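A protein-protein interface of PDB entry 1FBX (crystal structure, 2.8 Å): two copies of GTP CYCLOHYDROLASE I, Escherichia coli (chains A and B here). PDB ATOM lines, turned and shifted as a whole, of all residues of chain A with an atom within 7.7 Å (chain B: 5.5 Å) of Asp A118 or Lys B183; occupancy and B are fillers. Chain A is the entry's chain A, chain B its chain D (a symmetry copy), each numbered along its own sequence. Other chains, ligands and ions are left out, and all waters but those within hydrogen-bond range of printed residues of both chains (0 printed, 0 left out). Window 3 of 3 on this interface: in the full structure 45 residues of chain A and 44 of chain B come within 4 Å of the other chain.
The guanidinium group of Arg B188 sits at hydrogen-bond distance from the side-chain hydroxyl of Thr A107, 3.5 Å away.
The side-chain carboxylate of Asp A118 lies within hydrogen-bond range of the side-chain hydroxyl of Tyr B180 (2.8 Å).
The side-chain amino group (NZ) of Lys B183 lies within salt-bridge range of the side-chain carboxylate (OD2) of Asp A118, 2.8 Å away.
NE2 of Gln A142 sits close to NH1 of Arg B188 (3.2 Å).
The side-chain hydroxyl of Tyr A180 lies within hydrogen-bond range of the side-chain hydroxyl of Tyr B180, 3.0 Å away.
O of Thr A116 is in hydrogen-bond range of N of Tyr A180 (3.0 Å).
N of Val A178 sits at hydrogen-bond distance from O of Asp A118 (2.9 Å).
O of Val B182 lies within hydrogen-bond range of N of Arg B188.
The backbone carbonyl oxygen of Ala B184 sits at hydrogen-bond distance from the guanidinium group of Arg B188 (3.1 Å).
Printed residues of chain B that touch a printed residue of chain A: Tyr B180, Lys B183, Ala B184 and Arg B188.
Among the printed residues, Asp or Glu carboxylates within 4 Å of a Lys or Arg side-chain nitrogen of the other chain: Asp A118 with Lys B183 (2.8 Å).
Among the printed residues, pairs that only touch across the chains: Thr A107 with Ala B184 (3.7 Å) and Thr A116 with Tyr B180 (3.4 Å).
Printed residues of chain A within 4 Å of Tyr B180: Thr A116 (3.4 Å), Asp A118 (2.8 Å) and Tyr A180 (3.0 Å).
Printed residues of chain B within 4 Å of Gln A142: Arg B188 (3.2 Å).
Of the printed residues of chain A, Arg B188 touches Thr A107 (3.5 Å) and Gln A142 (3.2 Å).
Arg B185 touches none of the printed residues of chain A.
Cys B181 touches none of the printed residues of chain A.
The nearest printed residue of chain B that does not touch Asp A118 is Val B178 (6.5 Å).
The nearest residue of chain A that does not touch Lys B183 is Thr A107 (4.7 Å).
Tyr B180 touches its own counterpart, Tyr A180.
Positions printed for both chains: 178, 179 and 180.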
ATOM      1  N   THR A 105     -25.223   6.057 -15.949  1.00  0.00           N
ATOM      2  CA  THR A 105     -25.639   6.850 -17.105  1.00  0.00           C
ATOM      3  C   THR A 105     -26.960   7.559 -16.802  1.00  0.00           C
ATOM      4  O   THR A 105     -27.949   6.919 -16.431  1.00  0.00           O
ATOM      5  CB  THR A 105     -25.904   5.983 -18.307  1.00  0.00           C
ATOM      6  OG1 THR A 105     -24.669   5.559 -18.881  1.00  0.00           O
ATOM      7  CG2 THR A 105     -26.713   6.744 -19.323  1.00  0.00           C
ATOM      8  N   LEU A 106     -26.989   8.878 -16.981  1.00  0.00           N
ATOM      9  CA  LEU A 106     -28.196   9.645 -16.713  1.00  0.00           C
ATOM     10  C   LEU A 106     -28.489  10.637 -17.808  1.00  0.00           C
ATOM     11  O   LEU A 106     -27.711  11.543 -18.047  1.00  0.00           O
ATOM     12  CB  LEU A 106     -28.058  10.386 -15.387  1.00  0.00           C
ATOM     13  CG  LEU A 106     -29.084  11.451 -15.006  1.00  0.00           C
ATOM     14  CD1 LEU A 106     -29.002  11.734 -13.503  1.00  0.00           C
ATOM     15  CD2 LEU A 106     -28.811  12.718 -15.785  1.00  0.00           C
ATOM     16  N   THR A 107     -29.616  10.452 -18.481  1.00  0.00           N
ATOM     17  CA  THR A 107     -30.061  11.382 -19.517  1.00  0.00           C
ATOM     18  C   THR A 107     -31.446  11.870 -19.089  1.00  0.00           C
ATOM     19  O   THR A 107     -32.356  11.066 -18.961  1.00  0.00           O
ATOM     20  CB  THR A 107     -30.185  10.688 -20.828  1.00  0.00           C
ATOM     21  OG1 THR A 107     -31.032   9.553 -20.672  1.00  0.00           O
ATOM     22  CG2 THR A 107     -28.838  10.221 -21.277  1.00  0.00           C
ATOM     23  N   SER A 108     -31.609  13.167 -18.852  1.00  0.00           N
ATOM     24  CA  SER A 108     -32.898  13.693 -18.434  1.00  0.00           C
ATOM     25  C   SER A 108     -33.290  14.850 -19.376  1.00  0.00           C
ATOM     26  O   SER A 108     -32.744  14.957 -20.473  1.00  0.00           O
ATOM     27  CB  SER A 108     -32.798  14.139 -16.975  1.00  0.00           C
ATOM     28  OG  SER A 108     -34.025  14.646 -16.469  1.00  0.00           O
ATOM     29  N   THR A 109     -34.239  15.694 -18.973  1.00  0.00           N
ATOM     30  CA  THR A 109     -34.681  16.818 -19.802  1.00  0.00           C
ATOM     31  C   THR A 109     -34.828  18.052 -18.895  1.00  0.00           C
ATOM     32  O   THR A 109     -35.347  17.876 -17.807  1.00  0.00           O
ATOM     33  CB  THR A 109     -36.076  16.517 -20.377  1.00  0.00           C
ATOM     34  OG1 THR A 109     -36.049  15.346 -21.195  1.00  0.00           O
ATOM     35  CG2 THR A 109     -36.551  17.665 -21.197  1.00  0.00           C
ATOM     36  N   VAL A 115     -35.260  20.529 -23.122  1.00  0.00           N
ATOM     37  CA  VAL A 115     -34.074  20.172 -23.899  1.00  0.00           C
ATOM     38  C   VAL A 115     -33.213  19.097 -23.144  1.00  0.00           C
ATOM     39  O   VAL A 115     -33.260  18.963 -21.912  1.00  0.00           O
ATOM     40  CB  VAL A 115     -33.242  21.435 -24.190  1.00  0.00           C
ATOM     41  CG1 VAL A 115     -31.960  21.066 -24.897  1.00  0.00           C
ATOM     42  CG2 VAL A 115     -34.028  22.380 -25.037  1.00  0.00           C
ATOM     43  N   THR A 116     -32.441  18.321 -23.889  1.00  0.00           N
ATOM     44  CA  THR A 116     -31.617  17.253 -23.328  1.00  0.00           C
ATOM     45  C   THR A 116     -30.657  17.599 -22.212  1.00  0.00           C
ATOM     46  O   THR A 116     -29.966  18.598 -22.287  1.00  0.00           O
ATOM     47  CB  THR A 116     -30.746  16.620 -24.416  1.00  0.00           C
ATOM     48  OG1 THR A 116     -31.571  16.146 -25.485  1.00  0.00           O
ATOM     49  CG2 THR A 116     -29.941  15.485 -23.844  1.00  0.00           C
ATOM     50  N   ILE A 117     -30.610  16.757 -21.186  1.00  0.00           N
ATOM     51  CA  ILE A 117     -29.650  16.912 -20.089  1.00  0.00           C
ATOM     52  C   ILE A 117     -28.844  15.594 -20.090  1.00  0.00           C
ATOM     53  O   ILE A 117     -29.384  14.521 -19.821  1.00  0.00           O
ATOM     54  CB  ILE A 117     -30.296  17.037 -18.692  1.00  0.00           C
ATOM     55  CG1 ILE A 117     -30.939  18.401 -18.500  1.00  0.00           C
ATOM     56  CG2 ILE A 117     -29.226  16.839 -17.624  1.00  0.00           C
ATOM     57  CD1 ILE A 117     -31.450  18.602 -17.070  1.00  0.00           C
ATOM     58  N   ASP A 118     -27.559  15.661 -20.394  1.00  0.00           N
ATOM     59  CA  ASP A 118     -26.767  14.451 -20.425  1.00  0.00           C
ATOM     60  C   ASP A 118     -25.724  14.479 -19.314  1.00  0.00           C
ATOM     61  O   ASP A 118     -24.939  15.418 -19.217  1.00  0.00           O
ATOM     62  CB  ASP A 118     -26.113  14.343 -21.777  1.00  0.00           C
ATOM     63  CG  ASP A 118     -25.369  13.085 -21.930  1.00  0.00           C
ATOM     64  OD1 ASP A 118     -25.521  12.206 -21.054  1.00  0.00           O
ATOM     65  OD2 ASP A 118     -24.637  12.964 -22.925  1.00  0.00           O
ATOM     66  N   GLY A 119     -25.729  13.466 -18.455  1.00  0.00           N
ATOM     67  CA  GLY A 119     -24.780  13.445 -17.353  1.00  0.00           C
ATOM     68  C   GLY A 119     -24.455  12.074 -16.786  1.00  0.00           C
ATOM     69  O   GLY A 119     -24.743  11.033 -17.404  1.00  0.00           O
ATOM     70  N   LYS A 120     -23.849  12.080 -15.601  1.00  0.00           N
ATOM     71  CA  LYS A 120     -23.458  10.854 -14.908  1.00  0.00           C
ATOM     72  C   LYS A 120     -23.811  10.971 -13.434  1.00  0.00           C
ATOM     73  O   LYS A 120     -23.716  12.061 -12.841  1.00  0.00           O
ATOM     74  CB  LYS A 120     -21.946  10.653 -15.016  1.00  0.00           C
ATOM     75  CG  LYS A 120     -21.510   9.487 -15.818  1.00  0.00           C
ATOM     76  CD  LYS A 120     -21.815   9.688 -17.272  1.00  0.00           C
ATOM     77  CE  LYS A 120     -21.207   8.589 -18.135  1.00  0.00           C
ATOM     78  NZ  LYS A 120     -19.697   8.543 -17.998  1.00  0.00           N
ATOM     79  N   GLN A 142     -32.555   6.252 -13.196  1.00  0.00           N
ATOM     80  CA  GLN A 142     -33.131   6.571 -14.484  1.00  0.00           C
ATOM     81  C   GLN A 142     -34.636   6.811 -14.412  1.00  0.00           C
ATOM     82  O   GLN A 142     -35.211   7.400 -15.318  1.00  0.00           O
ATOM     83  CB  GLN A 142     -32.800   5.485 -15.523  1.00  0.00           C
ATOM     84  CG  GLN A 142     -31.425   5.663 -16.231  1.00  0.00           C
ATOM     85  CD  GLN A 142     -31.333   6.940 -17.107  1.00  0.00           C
ATOM     86  OE1 GLN A 142     -31.436   8.071 -16.608  1.00  0.00           O
ATOM     87  NE2 GLN A 142     -31.138   6.750 -18.418  1.00  0.00           N
ATOM     88  N   GLN A 151     -31.932  19.884 -11.942  1.00  0.00           N
ATOM     89  CA  GLN A 151     -30.884  19.080 -11.325  1.00  0.00           C
ATOM     90  C   GLN A 151     -30.868  19.079  -9.814  1.00  0.00           C
ATOM     91  O   GLN A 151     -30.585  18.054  -9.184  1.00  0.00           O
ATOM     92  CB  GLN A 151     -29.523  19.470 -11.846  1.00  0.00           C
ATOM     93  CG  GLN A 151     -28.575  18.334 -11.680  1.00  0.00           C
ATOM     94  CD  GLN A 151     -27.274  18.565 -12.374  1.00  0.00           C
ATOM     95  OE1 GLN A 151     -27.245  19.039 -13.511  1.00  0.00           O
ATOM     96  NE2 GLN A 151     -26.174  18.218 -11.705  1.00  0.00           N
ATOM     97  N   ILE A 175     -24.609  14.215  -8.829  1.00  0.00           N
ATOM     98  CA  ILE A 175     -24.843  14.194 -10.262  1.00  0.00           C
ATOM     99  C   ILE A 175     -24.024  15.298 -10.911  1.00  0.00           C
ATOM    100  O   ILE A 175     -23.852  16.388 -10.361  1.00  0.00           O
ATOM    101  CB  ILE A 175     -26.305  14.392 -10.576  1.00  0.00           C
ATOM    102  CG1 ILE A 175     -27.100  13.234  -9.960  1.00  0.00           C
ATOM    103  CG2 ILE A 175     -26.483  14.562 -12.075  1.00  0.00           C
ATOM    104  CD1 ILE A 175     -28.606  13.331 -10.140  1.00  0.00           C
ATOM    105  N   ASP A 176     -23.528  15.008 -12.100  1.00  0.00           N
ATOM    106  CA  ASP A 176     -22.671  15.937 -12.810  1.00  0.00           C
ATOM    107  C   ASP A 176     -23.207  15.923 -14.222  1.00  0.00           C
ATOM    108  O   ASP A 176     -23.219  14.878 -14.859  1.00  0.00           O
ATOM    109  CB  ASP A 176     -21.249  15.384 -12.743  1.00  0.00           C
ATOM    110  CG  ASP A 176     -20.229  16.336 -13.249  1.00  0.00           C
ATOM    111  OD1 ASP A 176     -19.841  17.257 -12.496  1.00  0.00           O
ATOM    112  OD2 ASP A 176     -19.824  16.151 -14.414  1.00  0.00           O
ATOM    113  N   ALA A 177     -23.665  17.060 -14.723  1.00  0.00           N
ATOM    114  CA  ALA A 177     -24.248  17.039 -16.053  1.00  0.00           C
ATOM    115  C   ALA A 177     -24.170  18.290 -16.911  1.00  0.00           C
ATOM    116  O   ALA A 177     -23.868  19.396 -16.443  1.00  0.00           O
ATOM    117  CB  ALA A 177     -25.700  16.611 -15.950  1.00  0.00           C
ATOM    118  N   VAL A 178     -24.482  18.074 -18.183  1.00  0.00           N
ATOM    119  CA  VAL A 178     -24.489  19.112 -19.188  1.00  0.00           C
ATOM    120  C   VAL A 178     -25.925  19.406 -19.597  1.00  0.00           C
ATOM    121  O   VAL A 178     -26.635  18.509 -20.065  1.00  0.00           O
ATOM    122  CB  VAL A 178     -23.708  18.658 -20.443  1.00  0.00           C
ATOM    123  CG1 VAL A 178     -23.896  19.651 -21.574  1.00  0.00           C
ATOM    124  CG2 VAL A 178     -22.271  18.520 -20.116  1.00  0.00           C
ATOM    125  N   HIS A 179     -26.341  20.659 -19.425  1.00  0.00           N
ATOM    126  CA  HIS A 179     -27.673  21.096 -19.811  1.00  0.00           C
ATOM    127  C   HIS A 179     -27.556  21.672 -21.202  1.00  0.00           C
ATOM    128  O   HIS A 179     -26.879  22.667 -21.402  1.00  0.00           O
ATOM    129  CB  HIS A 179     -28.164  22.166 -18.840  1.00  0.00           C
ATOM    130  CG  HIS A 179     -28.304  21.667 -17.436  1.00  0.00           C
ATOM    131  ND1 HIS A 179     -29.509  21.640 -16.765  1.00  0.00           N
ATOM    132  CD2 HIS A 179     -27.395  21.108 -16.603  1.00  0.00           C
ATOM    133  CE1 HIS A 179     -29.337  21.083 -15.581  1.00  0.00           C
ATOM    134  NE2 HIS A 179     -28.064  20.751 -15.459  1.00  0.00           N
ATOM    135  N   TYR A 180     -28.176  21.036 -22.180  1.00  0.00           N
ATOM    136  CA  TYR A 180     -28.123  21.569 -23.528  1.00  0.00           C
ATOM    137  C   TYR A 180     -28.804  22.890 -23.795  1.00  0.00           C
ATOM    138  O   TYR A 180     -28.568  23.490 -24.861  1.00  0.00           O
ATOM    139  CB  TYR A 180     -28.653  20.569 -24.535  1.00  0.00           C
ATOM    140  CG  TYR A 180     -27.579  19.635 -24.895  1.00  0.00           C
ATOM    141  CD1 TYR A 180     -27.360  18.510 -24.125  1.00  0.00           C
ATOM    142  CD2 TYR A 180     -26.696  19.927 -25.941  1.00  0.00           C
ATOM    143  CE1 TYR A 180     -26.302  17.702 -24.363  1.00  0.00           C
ATOM    144  CE2 TYR A 180     -25.632  19.128 -26.191  1.00  0.00           C
ATOM    145  CZ  TYR A 180     -25.434  18.008 -25.392  1.00  0.00           C
ATOM    146  OH  TYR A 180     -24.359  17.176 -25.591  1.00  0.00           O
ATOM    147  N   ALA A 193     -20.344  22.547 -17.037  1.00  0.00           N
ATOM    148  CA  ALA A 193     -21.139  21.417 -16.566  1.00  0.00           C
ATOM    149  C   ALA A 193     -21.501  21.722 -15.118  1.00  0.00           C
ATOM    150  O   ALA A 193     -20.768  22.451 -14.444  1.00  0.00           O
ATOM    151  CB  ALA A 193     -20.364  20.169 -16.644  1.00  0.00           C
ATOM    152  N   THR A 194     -22.621  21.176 -14.641  1.00  0.00           N
ATOM    153  CA  THR A 194     -23.068  21.434 -13.277  1.00  0.00           C
ATOM    154  C   THR A 194     -23.004  20.239 -12.354  1.00  0.00           C
ATOM    155  O   THR A 194     -23.404  19.129 -12.718  1.00  0.00           O
ATOM    156  CB  THR A 194     -24.513  21.960 -13.269  1.00  0.00           C
ATOM    157  OG1 THR A 194     -24.532  23.291 -13.782  1.00  0.00           O
ATOM    158  CG2 THR A 194     -25.055  22.006 -11.883  1.00  0.00           C
ATOM    159  N   VAL B 178     -23.571  13.289 -32.669  1.00  0.00           N
ATOM    160  CA  VAL B 178     -24.266  12.403 -31.775  1.00  0.00           C
ATOM    161  C   VAL B 178     -25.756  12.746 -31.718  1.00  0.00           C
ATOM    162  O   VAL B 178     -26.128  13.886 -31.517  1.00  0.00           O
ATOM    163  CB  VAL B 178     -23.638  12.484 -30.402  1.00  0.00           C
ATOM    164  CG1 VAL B 178     -24.662  12.172 -29.331  1.00  0.00           C
ATOM    165  CG2 VAL B 178     -22.502  11.524 -30.352  1.00  0.00           C
ATOM    166  N   HIS B 179     -26.608  11.747 -31.925  1.00  0.00           N
ATOM    167  CA  HIS B 179     -28.066  11.941 -31.903  1.00  0.00           C
ATOM    168  C   HIS B 179     -28.618  11.459 -30.580  1.00  0.00           C
ATOM    169  O   HIS B 179     -28.573  10.264 -30.288  1.00  0.00           O
ATOM    170  CB  HIS B 179     -28.736  11.166 -33.038  1.00  0.00           C
ATOM    171  CG  HIS B 179     -28.344  11.649 -34.404  1.00  0.00           C
ATOM    172  ND1 HIS B 179     -29.266  12.000 -35.362  1.00  0.00           N
ATOM    173  CD2 HIS B 179     -27.128  11.825 -34.971  1.00  0.00           C
ATOM    174  CE1 HIS B 179     -28.636  12.371 -36.462  1.00  0.00           C
ATOM    175  NE2 HIS B 179     -27.340  12.272 -36.250  1.00  0.00           N
ATOM    176  N   TYR B 180     -29.126  12.386 -29.773  1.00  0.00           N
ATOM    177  CA  TYR B 180     -29.657  12.006 -28.486  1.00  0.00           C
ATOM    178  C   TYR B 180     -30.903  11.181 -28.594  1.00  0.00           C
ATOM    179  O   TYR B 180     -31.349  10.612 -27.600  1.00  0.00           O
ATOM    180  CB  TYR B 180     -29.916  13.224 -27.609  1.00  0.00           C
ATOM    181  CG  TYR B 180     -28.667  13.614 -26.903  1.00  0.00           C
ATOM    182  CD1 TYR B 180     -27.724  14.407 -27.551  1.00  0.00           C
ATOM    183  CD2 TYR B 180     -28.335  13.063 -25.662  1.00  0.00           C
ATOM    184  CE1 TYR B 180     -26.475  14.637 -27.001  1.00  0.00           C
ATOM    185  CE2 TYR B 180     -27.075  13.288 -25.102  1.00  0.00           C
ATOM    186  CZ  TYR B 180     -26.158  14.074 -25.793  1.00  0.00           C
ATOM    187  OH  TYR B 180     -24.895  14.281 -25.338  1.00  0.00           O
ATOM    188  N   CYS B 181     -31.480  11.115 -29.792  1.00  0.00           N
ATOM    189  CA  CYS B 181     -32.671  10.301 -29.968  1.00  0.00           C
ATOM    190  C   CYS B 181     -32.226   8.849 -30.175  1.00  0.00           C
ATOM    191  O   CYS B 181     -33.048   7.965 -30.386  1.00  0.00           O
ATOM    192  CB  CYS B 181     -33.518  10.788 -31.146  1.00  0.00           C
ATOM    193  SG  CYS B 181     -32.904  10.251 -32.708  1.00  0.00           S
ATOM    194  N   VAL B 182     -30.920   8.607 -30.113  1.00  0.00           N
ATOM    195  CA  VAL B 182     -30.380   7.270 -30.247  1.00  0.00           C
ATOM    196  C   VAL B 182     -29.730   6.963 -28.920  1.00  0.00           C
ATOM    197  O   VAL B 182     -29.647   5.817 -28.474  1.00  0.00           O
ATOM    198  CB  VAL B 182     -29.308   7.194 -31.329  1.00  0.00           C
ATOM    199  CG1 VAL B 182     -28.670   5.799 -31.367  1.00  0.00           C
ATOM    200  CG2 VAL B 182     -29.916   7.482 -32.646  1.00  0.00           C
ATOM    201  N   LYS B 183     -29.285   8.007 -28.255  1.00  0.00           N
ATOM    202  CA  LYS B 183     -28.619   7.800 -26.995  1.00  0.00           C
ATOM    203  C   LYS B 183     -29.499   7.788 -25.785  1.00  0.00           C
ATOM    204  O   LYS B 183     -29.408   6.886 -24.990  1.00  0.00           O
ATOM    205  CB  LYS B 183     -27.545   8.855 -26.807  1.00  0.00           C
ATOM    206  CG  LYS B 183     -26.919   8.814 -25.463  1.00  0.00           C
ATOM    207  CD  LYS B 183     -25.794   9.779 -25.393  1.00  0.00           C
ATOM    208  CE  LYS B 183     -25.082   9.617 -24.090  1.00  0.00           C
ATOM    209  NZ  LYS B 183     -23.969  10.574 -24.118  1.00  0.00           N
ATOM    210  N   ALA B 184     -30.351   8.799 -25.657  1.00  0.00           N
ATOM    211  CA  ALA B 184     -31.230   8.978 -24.501  1.00  0.00           C
ATOM    212  C   ALA B 184     -32.558   8.265 -24.487  1.00  0.00           C
ATOM    213  O   ALA B 184     -33.253   8.293 -23.491  1.00  0.00           O
ATOM    214  CB  ALA B 184     -31.479  10.444 -24.309  1.00  0.00           C
ATOM    215  N   ARG B 185     -32.931   7.638 -25.586  1.00  0.00           N
ATOM    216  CA  ARG B 185     -34.204   6.949 -25.651  1.00  0.00           C
ATOM    217  C   ARG B 185     -34.131   5.934 -26.785  1.00  0.00           C
ATOM    218  O   ARG B 185     -33.208   5.988 -27.590  1.00  0.00           O
ATOM    219  CB  ARG B 185     -35.305   7.985 -25.862  1.00  0.00           C
ATOM    220  CG  ARG B 185     -36.343   7.606 -26.851  1.00  0.00           C
ATOM    221  CD  ARG B 185     -36.292   8.510 -28.044  1.00  0.00           C
ATOM    222  NE  ARG B 185     -36.144   7.731 -29.253  1.00  0.00           N
ATOM    223  CZ  ARG B 185     -36.961   6.744 -29.603  1.00  0.00           C
ATOM    224  NH1 ARG B 185     -37.993   6.437 -28.832  1.00  0.00           N
ATOM    225  NH2 ARG B 185     -36.724   6.034 -30.704  1.00  0.00           N
ATOM    226  N   ARG B 188     -31.026   3.389 -26.958  1.00  0.00           N
ATOM    227  CA  ARG B 188     -30.157   3.927 -25.920  1.00  0.00           C
ATOM    228  C   ARG B 188     -28.673   3.570 -26.067  1.00  0.00           C
ATOM    229  O   ARG B 188     -28.047   3.124 -25.113  1.00  0.00           O
ATOM    230  CB  ARG B 188     -30.651   3.486 -24.543  1.00  0.00           C
ATOM    231  CG  ARG B 188     -31.889   4.186 -24.076  1.00  0.00           C
ATOM    232  CD  ARG B 188     -32.324   3.687 -22.708  1.00  0.00           C
ATOM    233  NE  ARG B 188     -33.219   4.640 -22.039  1.00  0.00           N
ATOM    234  CZ  ARG B 188     -32.842   5.826 -21.531  1.00  0.00           C
ATOM    235  NH1 ARG B 188     -31.565   6.237 -21.597  1.00  0.00           N
ATOM    236  NH2 ARG B 188     -33.753   6.615 -20.954  1.00  0.00           N
ATOM    237  N   ASP B 189     -28.109   3.768 -27.254  1.00  0.00           N
ATOM    238  CA  ASP B 189     -26.693   3.495 -27.463  1.00  0.00           C
ATOM    239  C   ASP B 189     -25.919   4.717 -26.947  1.00  0.00           C
ATOM    240  O   ASP B 189     -26.058   5.827 -27.469  1.00  0.00           O
ATOM    241  CB  ASP B 189     -26.381   3.280 -28.955  1.00  0.00           C
ATOM    242  CG  ASP B 189     -25.001   2.658 -29.182  1.00  0.00           C
ATOM    243  OD1 ASP B 189     -24.025   3.152 -28.558  1.00  0.00           O
ATOM    244  OD2 ASP B 189     -24.896   1.683 -29.978  1.00  0.00           O
ATOM    245  N   ALA B 190     -25.096   4.518 -25.930  1.00  0.00           N
ATOM    246  CA  ALA B 190     -24.350   5.627 -25.379  1.00  0.00           C
ATOM    247  C   ALA B 190     -23.030   5.904 -26.077  1.00  0.00           C
ATOM    248  O   ALA B 190     -22.431   6.959 -25.876  1.00  0.00           O
ATOM    249  CB  ALA B 190     -24.100   5.396 -23.943  1.00  0.00           C
